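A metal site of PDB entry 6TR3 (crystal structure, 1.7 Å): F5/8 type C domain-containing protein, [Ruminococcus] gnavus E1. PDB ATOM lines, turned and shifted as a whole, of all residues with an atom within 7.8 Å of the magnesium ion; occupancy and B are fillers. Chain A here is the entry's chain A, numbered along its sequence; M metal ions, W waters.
Water W1 bridges OD2 of Asp 74 (3.3 Å) and ND2 of Asn 121 (3.4 Å). Water W3 lies within hydrogen-bond range of the side-chain carboxylate of Glu 78 and the backbone NH of Ala 77.
N of Phe 75 lies within hydrogen-bond range of OH of Tyr 119, 2.9 Å away. OD2 of Asp 74 lies within hydrogen-bond range of N of Lys 122 (3.0 Å). The side-chain carboxylate (OE2) of Glu 131 is in hydrogen-bond range of the side-chain hydroxyl (OH) of Tyr 119 (2.6 Å).
The magnesium ion is bound by O of Phe 75 (2.1 Å), OD1 of Asp 74 (2.1 Å), water W1 (2.1 Å), water W2 (2.1 Å), water W3 (2.1 Å) and OE1 of Glu 131 (2.1 Å).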
ATOM      1  N   ASN A  73      -8.491  -9.530  -0.935  1.00  0.00           N
ATOM      2  CA  ASN A  73      -9.927  -9.513  -0.728  1.00  0.00           C
ATOM      3  C   ASN A  73     -10.509 -10.902  -0.685  1.00  0.00           C
ATOM      4  O   ASN A  73     -10.021 -11.801  -1.372  1.00  0.00           O
ATOM      5  CB  ASN A  73     -10.600  -8.679  -1.813  1.00  0.00           C
ATOM      6  CG  ASN A  73     -10.116  -7.243  -1.836  1.00  0.00           C
ATOM      7  OD1 ASN A  73      -9.788  -6.683  -0.795  1.00  0.00           O
ATOM      8  ND2 ASN A  73     -10.061  -6.648  -3.016  1.00  0.00           N
ATOM      9  N   ASP A  74     -11.546 -11.071   0.125  1.00  0.00           N
ATOM     10  CA  ASP A  74     -12.354 -12.286   0.176  1.00  0.00           C
ATOM     11  C   ASP A  74     -12.872 -12.580  -1.231  1.00  0.00           C
ATOM     12  O   ASP A  74     -13.487 -11.719  -1.848  1.00  0.00           O
ATOM     13  CB  ASP A  74     -13.533 -12.055   1.132  1.00  0.00           C
ATOM     14  CG  ASP A  74     -14.309 -13.339   1.449  1.00  0.00           C
ATOM     15  OD1 ASP A  74     -14.383 -14.253   0.581  1.00  0.00           O
ATOM     16  OD2 ASP A  74     -14.842 -13.432   2.575  1.00  0.00           O
ATOM     17  N   PHE A  75     -12.587 -13.787  -1.726  1.00  0.00           N
ATOM     18  CA  PHE A  75     -13.051 -14.244  -3.048  1.00  0.00           C
ATOM     19  C   PHE A  75     -14.570 -14.195  -3.096  1.00  0.00           C
ATOM     20  O   PHE A  75     -15.249 -14.695  -2.214  1.00  0.00           O
ATOM     21  CB  PHE A  75     -12.549 -15.666  -3.317  1.00  0.00           C
ATOM     22  CG  PHE A  75     -12.829 -16.152  -4.716  1.00  0.00           C
ATOM     23  CD1 PHE A  75     -11.923 -15.903  -5.740  1.00  0.00           C
ATOM     24  CD2 PHE A  75     -13.971 -16.859  -5.009  1.00  0.00           C
ATOM     25  CE1 PHE A  75     -12.153 -16.327  -7.024  1.00  0.00           C
ATOM     26  CE2 PHE A  75     -14.223 -17.303  -6.299  1.00  0.00           C
ATOM     27  CZ  PHE A  75     -13.304 -17.043  -7.309  1.00  0.00           C
ATOM     28  N   ASP A  76     -15.113 -13.585  -4.150  1.00  0.00           N
ATOM     29  CA  ASP A  76     -16.561 -13.430  -4.289  1.00  0.00           C
ATOM     30  C   ASP A  76     -17.158 -14.515  -5.198  1.00  0.00           C
ATOM     31  O   ASP A  76     -17.418 -14.288  -6.381  1.00  0.00           O
ATOM     32  CB  ASP A  76     -16.899 -12.011  -4.771  1.00  0.00           C
ATOM     33  CG  ASP A  76     -18.416 -11.737  -4.798  1.00  0.00           C
ATOM     34  OD1 ASP A  76     -19.218 -12.616  -4.405  1.00  0.00           O
ATOM     35  OD2 ASP A  76     -18.799 -10.644  -5.239  1.00  0.00           O
ATOM     36  N   ALA A  77     -17.392 -15.691  -4.618  1.00  0.00           N
ATOM     37  CA  ALA A  77     -17.977 -16.840  -5.311  1.00  0.00           C
ATOM     38  C   ALA A  77     -19.443 -16.598  -5.647  1.00  0.00           C
ATOM     39  O   ALA A  77     -19.940 -16.992  -6.721  1.00  0.00           O
ATOM     40  CB  ALA A  77     -17.819 -18.104  -4.476  1.00  0.00           C
ATOM     41  N   GLU A  78     -20.133 -15.931  -4.722  1.00  0.00           N
ATOM     42  CA  GLU A  78     -21.571 -15.669  -4.810  1.00  0.00           C
ATOM     43  C   GLU A  78     -21.938 -14.949  -6.123  1.00  0.00           C
ATOM     44  O   GLU A  78     -22.773 -15.420  -6.895  1.00  0.00           O
ATOM     45  CB  GLU A  78     -21.971 -14.827  -3.580  1.00  0.00           C
ATOM     46  CG  GLU A  78     -21.975 -15.607  -2.254  1.00  0.00           C
ATOM     47  CD  GLU A  78     -20.590 -15.901  -1.642  1.00  0.00           C
ATOM     48  OE1 GLU A  78     -19.553 -15.282  -2.003  1.00  0.00           O
ATOM     49  OE2 GLU A  78     -20.565 -16.800  -0.763  1.00  0.00           O
ATOM     50  N   TYR A 119      -3.691 -15.869   2.213  1.00  0.00           N
ATOM     51  CA  TYR A 119      -5.069 -15.548   1.897  1.00  0.00           C
ATOM     52  C   TYR A 119      -5.991 -16.122   2.976  1.00  0.00           C
ATOM     53  O   TYR A 119      -5.808 -17.268   3.405  1.00  0.00           O
ATOM     54  CB  TYR A 119      -5.516 -16.112   0.540  1.00  0.00           C
ATOM     55  CG  TYR A 119      -7.028 -15.998   0.369  1.00  0.00           C
ATOM     56  CD1 TYR A 119      -7.624 -14.763   0.161  1.00  0.00           C
ATOM     57  CD2 TYR A 119      -7.855 -17.123   0.486  1.00  0.00           C
ATOM     58  CE1 TYR A 119      -8.989 -14.638   0.056  1.00  0.00           C
ATOM     59  CE2 TYR A 119      -9.241 -16.997   0.374  1.00  0.00           C
ATOM     60  CZ  TYR A 119      -9.801 -15.755   0.159  1.00  0.00           C
ATOM     61  OH  TYR A 119     -11.163 -15.582   0.034  1.00  0.00           O
ATOM     62  N   ASN A 121     -10.382 -15.621   4.015  1.00  0.00           N
ATOM     63  CA  ASN A 121     -11.692 -14.974   3.830  1.00  0.00           C
ATOM     64  C   ASN A 121     -12.141 -14.360   5.153  1.00  0.00           C
ATOM     65  O   ASN A 121     -11.407 -14.393   6.130  1.00  0.00           O
ATOM     66  CB  ASN A 121     -12.703 -15.952   3.197  1.00  0.00           C
ATOM     67  CG  ASN A 121     -13.226 -17.014   4.170  1.00  0.00           C
ATOM     68  OD1 ASN A 121     -12.838 -17.078   5.328  1.00  0.00           O
ATOM     69  ND2 ASN A 121     -14.135 -17.829   3.675  1.00  0.00           N
ATOM     70  N   LYS A 122     -13.362 -13.791   5.180  1.00  0.00           N
ATOM     71  CA  LYS A 122     -13.889 -13.100   6.363  1.00  0.00           C
ATOM     72  C   LYS A 122     -13.846 -13.972   7.623  1.00  0.00           C
ATOM     73  O   LYS A 122     -13.698 -13.455   8.730  1.00  0.00           O
ATOM     74  CB  LYS A 122     -15.333 -12.614   6.125  1.00  0.00           C
ATOM     75  CG  LYS A 122     -16.365 -13.738   6.009  1.00  0.00           C
ATOM     76  CD  LYS A 122     -17.802 -13.229   6.039  1.00  0.00           C
ATOM     77  CE  LYS A 122     -18.764 -14.356   5.690  1.00  0.00           C
ATOM     78  NZ  LYS A 122     -20.102 -13.821   5.320  1.00  0.00           N
ATOM     79  N   ASP A 127      -9.453 -21.447   1.331  1.00  0.00           N
ATOM     80  CA  ASP A 127      -9.824 -22.529   0.455  1.00  0.00           C
ATOM     81  C   ASP A 127     -10.797 -22.005  -0.569  1.00  0.00           C
ATOM     82  O   ASP A 127     -11.988 -21.859  -0.287  1.00  0.00           O
ATOM     83  CB  ASP A 127     -10.425 -23.664   1.299  1.00  0.00           C
ATOM     84  CG  ASP A 127     -10.541 -24.965   0.543  1.00  0.00           C
ATOM     85  OD1 ASP A 127     -10.893 -24.917  -0.647  1.00  0.00           O
ATOM     86  OD2 ASP A 127     -10.253 -26.023   1.142  1.00  0.00           O
ATOM     87  N   ILE A 128     -10.281 -21.698  -1.765  1.00  0.00           N
ATOM     88  CA  ILE A 128     -11.087 -21.105  -2.816  1.00  0.00           C
ATOM     89  C   ILE A 128     -12.081 -22.112  -3.351  1.00  0.00           C
ATOM     90  O   ILE A 128     -13.220 -21.783  -3.591  1.00  0.00           O
ATOM     91  CB  ILE A 128     -10.241 -20.533  -3.946  1.00  0.00           C
ATOM     92  CG1 ILE A 128      -9.239 -19.494  -3.392  1.00  0.00           C
ATOM     93  CG2 ILE A 128     -11.109 -19.922  -5.035  1.00  0.00           C
ATOM     94  CD1 ILE A 128      -9.866 -18.255  -2.781  1.00  0.00           C
ATOM     95  N   GLU A 131     -14.998 -22.253  -1.148  1.00  0.00           N
ATOM     96  CA  GLU A 131     -15.816 -21.040  -1.294  1.00  0.00           C
ATOM     97  C   GLU A 131     -16.742 -21.148  -2.507  1.00  0.00           C
ATOM     98  O   GLU A 131     -17.931 -20.787  -2.438  1.00  0.00           O
ATOM     99  CB  GLU A 131     -14.935 -19.806  -1.403  1.00  0.00           C
ATOM    100  CG  GLU A 131     -14.301 -19.368  -0.089  1.00  0.00           C
ATOM    101  CD  GLU A 131     -13.627 -18.000  -0.177  1.00  0.00           C
ATOM    102  OE1 GLU A 131     -14.299 -17.028  -0.581  1.00  0.00           O
ATOM    103  OE2 GLU A 131     -12.407 -17.897   0.159  1.00  0.00           O
ATOM    104  N   ILE A 132     -16.178 -21.611  -3.632  1.00  0.00           N
ATOM    105  CA  ILE A 132     -16.929 -21.791  -4.867  1.00  0.00           C
ATOM    106  C   ILE A 132     -17.970 -22.897  -4.686  1.00  0.00           C
ATOM    107  O   ILE A 132     -19.133 -22.752  -5.109  1.00  0.00           O
ATOM    108  CB  ILE A 132     -16.015 -22.077  -6.050  1.00  0.00           C
ATOM    109  CG1 ILE A 132     -15.144 -20.852  -6.315  1.00  0.00           C
ATOM    110  CG2 ILE A 132     -16.847 -22.326  -7.300  1.00  0.00           C
ATOM    111  CD1 ILE A 132     -14.009 -21.100  -7.269  1.00  0.00           C
ATOM    112  N   GLY A 348     -10.242 -11.052  -6.692  1.00  0.00           N
ATOM    113  CA  GLY A 348     -11.132 -12.163  -6.336  1.00  0.00           C
ATOM    114  C   GLY A 348     -12.586 -12.012  -6.745  1.00  0.00           C
ATOM    115  O   GLY A 348     -13.456 -12.766  -6.270  1.00  0.00           O
HETATM  116 MG    MG M   1     -15.729 -15.488  -0.377  1.00  0.00          MG
HETATM  117  O   HOH W   1     -16.144 -16.248   1.508  1.00  0.00           O
HETATM  118  O   HOH W   2     -17.105 -13.919  -0.239  1.00  0.00           O
HETATM  119  O   HOH W   3     -17.086 -16.702  -1.408  1.00  0.00           O
